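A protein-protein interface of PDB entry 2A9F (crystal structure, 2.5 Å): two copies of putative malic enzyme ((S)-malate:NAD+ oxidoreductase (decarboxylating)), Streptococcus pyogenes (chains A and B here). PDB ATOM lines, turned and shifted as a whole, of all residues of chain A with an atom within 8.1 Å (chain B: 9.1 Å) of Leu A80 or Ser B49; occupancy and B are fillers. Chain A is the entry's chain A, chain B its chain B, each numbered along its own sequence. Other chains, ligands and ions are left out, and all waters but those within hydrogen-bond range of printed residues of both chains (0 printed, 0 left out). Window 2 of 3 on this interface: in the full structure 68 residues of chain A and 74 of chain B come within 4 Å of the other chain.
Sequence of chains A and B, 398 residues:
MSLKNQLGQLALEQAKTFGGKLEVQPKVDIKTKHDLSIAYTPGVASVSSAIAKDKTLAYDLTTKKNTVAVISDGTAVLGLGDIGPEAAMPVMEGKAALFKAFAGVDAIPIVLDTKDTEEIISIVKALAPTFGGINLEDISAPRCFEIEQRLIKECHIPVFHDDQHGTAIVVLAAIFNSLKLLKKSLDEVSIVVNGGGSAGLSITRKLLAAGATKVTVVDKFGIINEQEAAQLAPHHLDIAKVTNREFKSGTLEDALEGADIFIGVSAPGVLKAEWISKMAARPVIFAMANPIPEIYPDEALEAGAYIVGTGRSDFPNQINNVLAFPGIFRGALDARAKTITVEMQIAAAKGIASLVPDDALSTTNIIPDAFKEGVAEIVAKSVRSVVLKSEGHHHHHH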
ATOM      1  N   LEU A  12      10.621   2.131 -20.421  1.00  0.00           N
ATOM      2  CA  LEU A  12      11.722   1.936 -19.501  1.00  0.00           C
ATOM      3  C   LEU A  12      11.228   0.646 -18.857  1.00  0.00           C
ATOM      4  O   LEU A  12      11.971  -0.093 -18.197  1.00  0.00           O
ATOM      5  CB  LEU A  12      11.730   3.090 -18.499  1.00  0.00           C
ATOM      6  CG  LEU A  12      12.723   3.230 -17.348  1.00  0.00           C
ATOM      7  CD1 LEU A  12      14.129   2.862 -17.764  1.00  0.00           C
ATOM      8  CD2 LEU A  12      12.674   4.664 -16.889  1.00  0.00           C
ATOM      9  N   GLY A  74      31.751   4.589 -20.095  1.00  0.00           N
ATOM     10  CA  GLY A  74      30.636   5.418 -19.672  1.00  0.00           C
ATOM     11  C   GLY A  74      30.951   6.896 -19.490  1.00  0.00           C
ATOM     12  O   GLY A  74      30.190   7.623 -18.845  1.00  0.00           O
ATOM     13  N   THR A  75      32.058   7.358 -20.063  1.00  0.00           N
ATOM     14  CA  THR A  75      32.428   8.770 -19.930  1.00  0.00           C
ATOM     15  C   THR A  75      31.772   9.686 -20.956  1.00  0.00           C
ATOM     16  O   THR A  75      31.707  10.897 -20.744  1.00  0.00           O
ATOM     17  CB  THR A  75      33.945   8.962 -20.037  1.00  0.00           C
ATOM     18  OG1 THR A  75      34.389   8.578 -21.351  1.00  0.00           O
ATOM     19  CG2 THR A  75      34.654   8.108 -18.983  1.00  0.00           C
ATOM     20  N   ALA A  76      31.289   9.110 -22.058  1.00  0.00           N
ATOM     21  CA  ALA A  76      30.655   9.878 -23.132  1.00  0.00           C
ATOM     22  C   ALA A  76      29.411   9.204 -23.720  1.00  0.00           C
ATOM     23  O   ALA A  76      29.205   9.179 -24.940  1.00  0.00           O
ATOM     24  CB  ALA A  76      31.668  10.146 -24.239  1.00  0.00           C
ATOM     25  N   VAL A  77      28.573   8.671 -22.845  1.00  0.00           N
ATOM     26  CA  VAL A  77      27.354   8.016 -23.283  1.00  0.00           C
ATOM     27  C   VAL A  77      26.361   8.983 -23.942  1.00  0.00           C
ATOM     28  O   VAL A  77      25.891   9.930 -23.315  1.00  0.00           O
ATOM     29  CB  VAL A  77      26.655   7.330 -22.100  1.00  0.00           C
ATOM     30  CG1 VAL A  77      25.471   6.513 -22.608  1.00  0.00           C
ATOM     31  CG2 VAL A  77      27.653   6.471 -21.339  1.00  0.00           C
ATOM     32  N   LEU A  78      26.053   8.722 -25.210  1.00  0.00           N
ATOM     33  CA  LEU A  78      25.107   9.519 -25.996  1.00  0.00           C
ATOM     34  C   LEU A  78      25.235  11.052 -25.876  1.00  0.00           C
ATOM     35  O   LEU A  78      26.285  11.627 -26.161  1.00  0.00           O
ATOM     36  CB  LEU A  78      23.668   9.081 -25.653  1.00  0.00           C
ATOM     37  CG  LEU A  78      22.996   7.926 -26.407  1.00  0.00           C
ATOM     38  CD1 LEU A  78      24.013   6.889 -26.798  1.00  0.00           C
ATOM     39  CD2 LEU A  78      21.908   7.303 -25.523  1.00  0.00           C
ATOM     40  N   GLY A  79      24.141  11.697 -25.479  1.00  0.00           N
ATOM     41  CA  GLY A  79      24.118  13.139 -25.329  1.00  0.00           C
ATOM     42  C   GLY A  79      24.060  13.503 -23.863  1.00  0.00           C
ATOM     43  O   GLY A  79      23.746  14.633 -23.496  1.00  0.00           O
ATOM     44  N   LEU A  80      24.346  12.520 -23.020  1.00  0.00           N
ATOM     45  CA  LEU A  80      24.368  12.715 -21.582  1.00  0.00           C
ATOM     46  C   LEU A  80      25.828  13.041 -21.266  1.00  0.00           C
ATOM     47  O   LEU A  80      26.440  13.844 -21.974  1.00  0.00           O
ATOM     48  CB  LEU A  80      23.924  11.428 -20.888  1.00  0.00           C
ATOM     49  CG  LEU A  80      22.545  10.922 -21.342  1.00  0.00           C
ATOM     50  CD1 LEU A  80      22.269   9.558 -20.740  1.00  0.00           C
ATOM     51  CD2 LEU A  80      21.460  11.919 -20.927  1.00  0.00           C
ATOM     52  N   GLY A  81      26.403  12.434 -20.233  1.00  0.00           N
ATOM     53  CA  GLY A  81      27.800  12.722 -19.939  1.00  0.00           C
ATOM     54  C   GLY A  81      28.499  11.570 -19.250  1.00  0.00           C
ATOM     55  O   GLY A  81      28.018  10.445 -19.299  1.00  0.00           O
ATOM     56  N   ASP A  82      29.638  11.823 -18.620  1.00  0.00           N
ATOM     57  CA  ASP A  82      30.322  10.749 -17.915  1.00  0.00           C
ATOM     58  C   ASP A  82      29.384  10.320 -16.793  1.00  0.00           C
ATOM     59  O   ASP A  82      29.378  10.915 -15.711  1.00  0.00           O
ATOM     60  CB  ASP A  82      31.660  11.236 -17.353  1.00  0.00           C
ATOM     61  CG  ASP A  82      32.345  10.197 -16.481  1.00  0.00           C
ATOM     62  OD1 ASP A  82      32.147   8.978 -16.709  1.00  0.00           O
ATOM     63  OD2 ASP A  82      33.097  10.612 -15.571  1.00  0.00           O
ATOM     64  N   ILE A  83      28.584   9.288 -17.074  1.00  0.00           N
ATOM     65  CA  ILE A  83      27.609   8.772 -16.131  1.00  0.00           C
ATOM     66  C   ILE A  83      28.009   7.443 -15.510  1.00  0.00           C
ATOM     67  O   ILE A  83      27.267   6.882 -14.700  1.00  0.00           O
ATOM     68  CB  ILE A  83      26.253   8.601 -16.810  1.00  0.00           C
ATOM     69  CG1 ILE A  83      26.401   7.729 -18.063  1.00  0.00           C
ATOM     70  CG2 ILE A  83      25.709   9.945 -17.203  1.00  0.00           C
ATOM     71  CD1 ILE A  83      25.093   7.438 -18.794  1.00  0.00           C
ATOM     72  N   ALA A  87      25.434   2.779 -15.931  1.00  0.00           N
ATOM     73  CA  ALA A  87      24.449   3.617 -16.623  1.00  0.00           C
ATOM     74  C   ALA A  87      24.613   3.553 -18.142  1.00  0.00           C
ATOM     75  O   ALA A  87      23.668   3.811 -18.886  1.00  0.00           O
ATOM     76  CB  ALA A  87      24.564   5.064 -16.150  1.00  0.00           C
ATOM     77  N   ALA A  88      25.809   3.198 -18.594  1.00  0.00           N
ATOM     78  CA  ALA A  88      26.079   3.104 -20.018  1.00  0.00           C
ATOM     79  C   ALA A  88      25.545   1.794 -20.633  1.00  0.00           C
ATOM     80  O   ALA A  88      25.102   1.774 -21.787  1.00  0.00           O
ATOM     81  CB  ALA A  88      27.583   3.210 -20.264  1.00  0.00           C
ATOM     82  N   PRO A  90      22.824   0.055 -20.845  1.00  0.00           N
ATOM     83  CA  PRO A  90      21.621   0.054 -21.690  1.00  0.00           C
ATOM     84  C   PRO A  90      21.954   0.431 -23.132  1.00  0.00           C
ATOM     85  O   PRO A  90      21.409  -0.144 -24.071  1.00  0.00           O
ATOM     86  CB  PRO A  90      20.723   1.097 -21.023  1.00  0.00           C
ATOM     87  CG  PRO A  90      21.091   0.973 -19.612  1.00  0.00           C
ATOM     88  CD  PRO A  90      22.598   0.871 -19.642  1.00  0.00           C
ATOM     89  N   VAL A  91      22.855   1.395 -23.297  1.00  0.00           N
ATOM     90  CA  VAL A  91      23.249   1.846 -24.625  1.00  0.00           C
ATOM     91  C   VAL A  91      24.181   0.855 -25.339  1.00  0.00           C
ATOM     92  O   VAL A  91      24.047   0.619 -26.539  1.00  0.00           O
ATOM     93  CB  VAL A  91      23.936   3.225 -24.554  1.00  0.00           C
ATOM     94  CG1 VAL A  91      24.439   3.640 -25.929  1.00  0.00           C
ATOM     95  CG2 VAL A  91      22.961   4.250 -24.019  1.00  0.00           C
ATOM     96  N   ASP A 138      31.261   5.514 -27.143  1.00  0.00           N
ATOM     97  CA  ASP A 138      31.015   6.580 -26.202  1.00  0.00           C
ATOM     98  C   ASP A 138      32.104   6.903 -25.179  1.00  0.00           C
ATOM     99  O   ASP A 138      31.794   7.196 -24.031  1.00  0.00           O
ATOM    100  CB  ASP A 138      29.690   6.318 -25.472  1.00  0.00           C
ATOM    101  CG  ASP A 138      28.499   6.275 -26.420  1.00  0.00           C
ATOM    102  OD1 ASP A 138      28.666   6.581 -27.630  1.00  0.00           O
ATOM    103  OD2 ASP A 138      27.391   5.938 -25.946  1.00  0.00           O
ATOM    104  N   PRO A 291      23.357  17.740 -30.924  1.00  0.00           N
ATOM    105  CA  PRO A 291      22.284  18.654 -30.533  1.00  0.00           C
ATOM    106  C   PRO A 291      22.154  19.903 -31.397  1.00  0.00           C
ATOM    107  O   PRO A 291      21.393  19.906 -32.365  1.00  0.00           O
ATOM    108  CB  PRO A 291      22.626  18.949 -29.078  1.00  0.00           C
ATOM    109  CG  PRO A 291      23.085  17.561 -28.582  1.00  0.00           C
ATOM    110  CD  PRO A 291      23.536  16.759 -29.839  1.00  0.00           C
ATOM    111  N   PRO B  42      15.965   7.555 -29.168  1.00  0.00           N
ATOM    112  CA  PRO B  42      16.355   8.309 -27.977  1.00  0.00           C
ATOM    113  C   PRO B  42      15.680   7.780 -26.708  1.00  0.00           C
ATOM    114  O   PRO B  42      15.759   8.400 -25.647  1.00  0.00           O
ATOM    115  CB  PRO B  42      15.861   9.704 -28.310  1.00  0.00           C
ATOM    116  CG  PRO B  42      14.491   9.373 -28.911  1.00  0.00           C
ATOM    117  CD  PRO B  42      14.760   8.150 -29.781  1.00  0.00           C
ATOM    118  N   GLY B  43      15.005   6.647 -26.827  1.00  0.00           N
ATOM    119  CA  GLY B  43      14.309   6.078 -25.688  1.00  0.00           C
ATOM    120  C   GLY B  43      15.248   5.486 -24.663  1.00  0.00           C
ATOM    121  O   GLY B  43      15.026   5.627 -23.457  1.00  0.00           O
ATOM    122  N   VAL B  44      16.296   4.817 -25.142  1.00  0.00           N
ATOM    123  CA  VAL B  44      17.255   4.209 -24.246  1.00  0.00           C
ATOM    124  C   VAL B  44      17.914   5.277 -23.351  1.00  0.00           C
ATOM    125  O   VAL B  44      18.443   4.960 -22.282  1.00  0.00           O
ATOM    126  CB  VAL B  44      18.329   3.427 -25.038  1.00  0.00           C
ATOM    127  CG1 VAL B  44      19.055   4.345 -25.975  1.00  0.00           C
ATOM    128  CG2 VAL B  44      19.298   2.750 -24.080  1.00  0.00           C
ATOM    129  N   ALA B  45      17.865   6.541 -23.769  1.00  0.00           N
ATOM    130  CA  ALA B  45      18.464   7.612 -22.977  1.00  0.00           C
ATOM    131  C   ALA B  45      17.803   7.752 -21.599  1.00  0.00           C
ATOM    132  O   ALA B  45      18.450   8.196 -20.641  1.00  0.00           O
ATOM    133  CB  ALA B  45      18.401   8.941 -23.742  1.00  0.00           C
ATOM    134  N   SER B  46      16.526   7.382 -21.492  1.00  0.00           N
ATOM    135  CA  SER B  46      15.841   7.453 -20.204  1.00  0.00           C
ATOM    136  C   SER B  46      16.312   6.326 -19.278  1.00  0.00           C
ATOM    137  O   SER B  46      16.291   6.464 -18.053  1.00  0.00           O
ATOM    138  CB  SER B  46      14.324   7.346 -20.376  1.00  0.00           C
ATOM    139  OG  SER B  46      13.801   8.462 -21.065  1.00  0.00           O
ATOM    140  N   VAL B  47      16.717   5.207 -19.875  1.00  0.00           N
ATOM    141  CA  VAL B  47      17.192   4.064 -19.105  1.00  0.00           C
ATOM    142  C   VAL B  47      18.562   4.375 -18.522  1.00  0.00           C
ATOM    143  O   VAL B  47      18.817   4.105 -17.344  1.00  0.00           O
ATOM    144  CB  VAL B  47      17.313   2.800 -19.970  1.00  0.00           C
ATOM    145  CG1 VAL B  47      17.817   1.642 -19.119  1.00  0.00           C
ATOM    146  CG2 VAL B  47      15.967   2.465 -20.593  1.00  0.00           C
ATOM    147  N   SER B  48      19.440   4.930 -19.353  1.00  0.00           N
ATOM    148  CA  SER B  48      20.778   5.296 -18.903  1.00  0.00           C
ATOM    149  C   SER B  48      20.699   6.306 -17.755  1.00  0.00           C
ATOM    150  O   SER B  48      21.305   6.113 -16.695  1.00  0.00           O
ATOM    151  CB  SER B  48      21.583   5.897 -20.055  1.00  0.00           C
ATOM    152  OG  SER B  48      21.937   4.898 -21.002  1.00  0.00           O
ATOM    153  N   SER B  49      19.924   7.364 -17.976  1.00  0.00           N
ATOM    154  CA  SER B  49      19.749   8.421 -16.994  1.00  0.00           C
ATOM    155  C   SER B  49      19.186   7.922 -15.677  1.00  0.00           C
ATOM    156  O   SER B  49      19.665   8.297 -14.595  1.00  0.00           O
ATOM    157  CB  SER B  49      18.851   9.519 -17.568  1.00  0.00           C
ATOM    158  OG  SER B  49      19.468  10.114 -18.701  1.00  0.00           O
ATOM    159  N   ALA B  50      18.171   7.075 -15.766  1.00  0.00           N
ATOM    160  CA  ALA B  50      17.563   6.537 -14.569  1.00  0.00           C
ATOM    161  C   ALA B  50      18.626   5.795 -13.765  1.00  0.00           C
ATOM    162  O   ALA B  50      18.749   5.980 -12.550  1.00  0.00           O
ATOM    163  CB  ALA B  50      16.421   5.604 -14.934  1.00  0.00           C
ATOM    164  N   ILE B  51      19.409   4.969 -14.446  1.00  0.00           N
ATOM    165  CA  ILE B  51      20.451   4.203 -13.783  1.00  0.00           C
ATOM    166  C   ILE B  51      21.532   5.128 -13.250  1.00  0.00           C
ATOM    167  O   ILE B  51      22.138   4.842 -12.219  1.00  0.00           O
ATOM    168  CB  ILE B  51      21.091   3.171 -14.748  1.00  0.00           C
ATOM    169  CG1 ILE B  51      20.093   2.061 -15.047  1.00  0.00           C
ATOM    170  CG2 ILE B  51      22.374   2.579 -14.139  1.00  0.00           C
ATOM    171  CD1 ILE B  51      20.577   1.124 -16.104  1.00  0.00           C
ATOM    172  N   ALA B  52      21.773   6.232 -13.955  1.00  0.00           N
ATOM    173  CA  ALA B  52      22.791   7.195 -13.538  1.00  0.00           C
ATOM    174  C   ALA B  52      22.447   7.806 -12.181  1.00  0.00           C
ATOM    175  O   ALA B  52      23.337   8.140 -11.397  1.00  0.00           O
ATOM    176  CB  ALA B  52      22.929   8.294 -14.573  1.00  0.00           C
ATOM    177  N   LYS B  53      21.151   7.930 -11.907  1.00  0.00           N
ATOM    178  CA  LYS B  53      20.666   8.506 -10.657  1.00  0.00           C
ATOM    179  C   LYS B  53      20.494   7.465  -9.546  1.00  0.00           C
ATOM    180  O   LYS B  53      20.453   7.808  -8.370  1.00  0.00           O
ATOM    181  CB  LYS B  53      19.323   9.202 -10.895  1.00  0.00           C
ATOM    182  CG  LYS B  53      19.312  10.218 -12.040  1.00  0.00           C
ATOM    183  CD  LYS B  53      17.920  10.845 -12.186  1.00  0.00           C
ATOM    184  CE  LYS B  53      17.836  11.802 -13.365  1.00  0.00           C
ATOM    185  NZ  LYS B  53      16.495  12.458 -13.446  1.00  0.00           N
ATOM    186  N   ASP B  54      20.375   6.198  -9.921  1.00  0.00           N
ATOM    187  CA  ASP B  54      20.199   5.119  -8.946  1.00  0.00           C
ATOM    188  C   ASP B  54      20.931   3.868  -9.423  1.00  0.00           C
ATOM    189  O   ASP B  54      20.393   3.084 -10.215  1.00  0.00           O
ATOM    190  CB  ASP B  54      18.715   4.789  -8.771  1.00  0.00           C
ATOM    191  CG  ASP B  54      18.475   3.764  -7.686  1.00  0.00           C
ATOM    192  OD1 ASP B  54      19.395   2.960  -7.417  1.00  0.00           O
ATOM    193  OD2 ASP B  54      17.371   3.756  -7.110  1.00  0.00           O
ATOM    194  N   LYS B  55      22.148   3.667  -8.931  1.00  0.00           N
ATOM    195  CA  LYS B  55      22.929   2.523  -9.356  1.00  0.00           C
ATOM    196  C   LYS B  55      22.336   1.145  -9.084  1.00  0.00           C
ATOM    197  O   LYS B  55      22.535   0.239  -9.884  1.00  0.00           O
ATOM    198  CB  LYS B  55      24.335   2.615  -8.785  1.00  0.00           C
ATOM    199  CG  LYS B  55      25.343   3.127  -9.791  1.00  0.00           C
ATOM    200  CD  LYS B  55      26.481   2.133  -9.970  1.00  0.00           C
ATOM    201  CE  LYS B  55      27.207   1.873  -8.646  1.00  0.00           C
ATOM    202  NZ  LYS B  55      28.500   1.103  -8.769  1.00  0.00           N
ATOM    203  N   LEU B  57      19.824   0.123  -9.766  1.00  0.00           N
ATOM    204  CA  LEU B  57      18.905  -0.164 -10.865  1.00  0.00           C
ATOM    205  C   LEU B  57      19.636  -0.963 -11.926  1.00  0.00           C
ATOM    206  O   LEU B  57      19.018  -1.569 -12.798  1.00  0.00           O
ATOM    207  CB  LEU B  57      18.366   1.124 -11.505  1.00  0.00           C
ATOM    208  CG  LEU B  57      17.391   1.985 -10.702  1.00  0.00           C
ATOM    209  CD1 LEU B  57      16.836   3.061 -11.612  1.00  0.00           C
ATOM    210  CD2 LEU B  57      16.260   1.133 -10.130  1.00  0.00           C
ATOM    211  N   LEU B  61      17.601  -2.986 -14.736  1.00  0.00           N
ATOM    212  CA  LEU B  61      17.402  -2.649 -16.152  1.00  0.00           C
ATOM    213  C   LEU B  61      18.457  -3.077 -17.181  1.00  0.00           C
ATOM    214  O   LEU B  61      18.327  -2.773 -18.379  1.00  0.00           O
ATOM    215  CB  LEU B  61      17.194  -1.136 -16.265  1.00  0.00           C
ATOM    216  CG  LEU B  61      16.307  -0.507 -15.185  1.00  0.00           C
ATOM    217  CD1 LEU B  61      16.493   1.010 -15.164  1.00  0.00           C
ATOM    218  CD2 LEU B  61      14.865  -0.888 -15.436  1.00  0.00           C
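The backbone carbonyl oxygen of Ala A87 is in hydrogen-bond range of the side-chain hydroxyl of Ser B48.
The backbone carbonyl oxygen (O) of Ala B45 lies within hydrogen-bond range of the side-chain hydroxyl (OG) of Ser B49, 2.9 Å away.
CD1 of Leu A12 touches CG2 of Val B47, at 3.4 Å.
Leu A12 touches Leu B61 (CD1 to CD1, 3.97 Å).
Ser B48 touches Leu A80.
Leu A80 touches Ser B49 (CD2 to OG, 3.5 Å).
N of Ala B52 touches CB of Ala A87, at 3.7 Å.
CG2 of Val B44 touches O of Pro A90, 3.6 Å away.
Pro A90 touches Ser B48 (CB to OG, 3.99 Å).
Ile B51 touches Pro A90.
CG2 of Val B44 touches N of Val A91 (3.9 Å).
Val A91 touches Ser B48 (CG2 to OG, 3.3 Å).
Of chain B, only Ser B48 (3.8 Å) and Ser B49 (3.5 Å) come within 4 Å of Leu A80.
Ser B49 touches one residue of chain A.
No residue of chain B comes within 4 Å of Gly A81.
No residue of chain A comes within 4 Å of Ala B50.
Of the printed residues of chain A, Ala B52 touches Ala A87 (3.7 Å).
Of the printed residues of chain B, Ala A87 touches Ser B48 (2.9 Å), Ile B51 (3.4 Å) and Ala B52 (3.7 Å).
Thr A75 touches none of the printed residues of chain B.
The nearest residue of chain B that does not touch Leu A80 is Ala B45 (4.1 Å).
Printed residues of chain B that touch a printed residue of chain A: Val B44, Val B47, Ser B48, Ser B49, Ile B51, Ala B52 and Leu B61.
Hydrophobic or aromatic side chains of chain B that line the printed part of chain A: Val B44, Val B47, Ile B51, Ala B52 and Leu B61.
Of the 17 printed residues of chain A, 5 touch a printed residue of chain B.
Hydrophobic or aromatic side chains of chain A that line the printed part of chain B: Leu A12, Leu A80, Ala A87, Pro A90 and Val A91.
Among the printed residues, no Asp or Glu carboxylate lies within 4 Å of a Lys or Arg side-chain nitrogen of the other chain.
No position is printed for both chains.
Of the 13 pairs that touch across the chains among the printed residues, none has its exchanged pair printed and touching as well.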
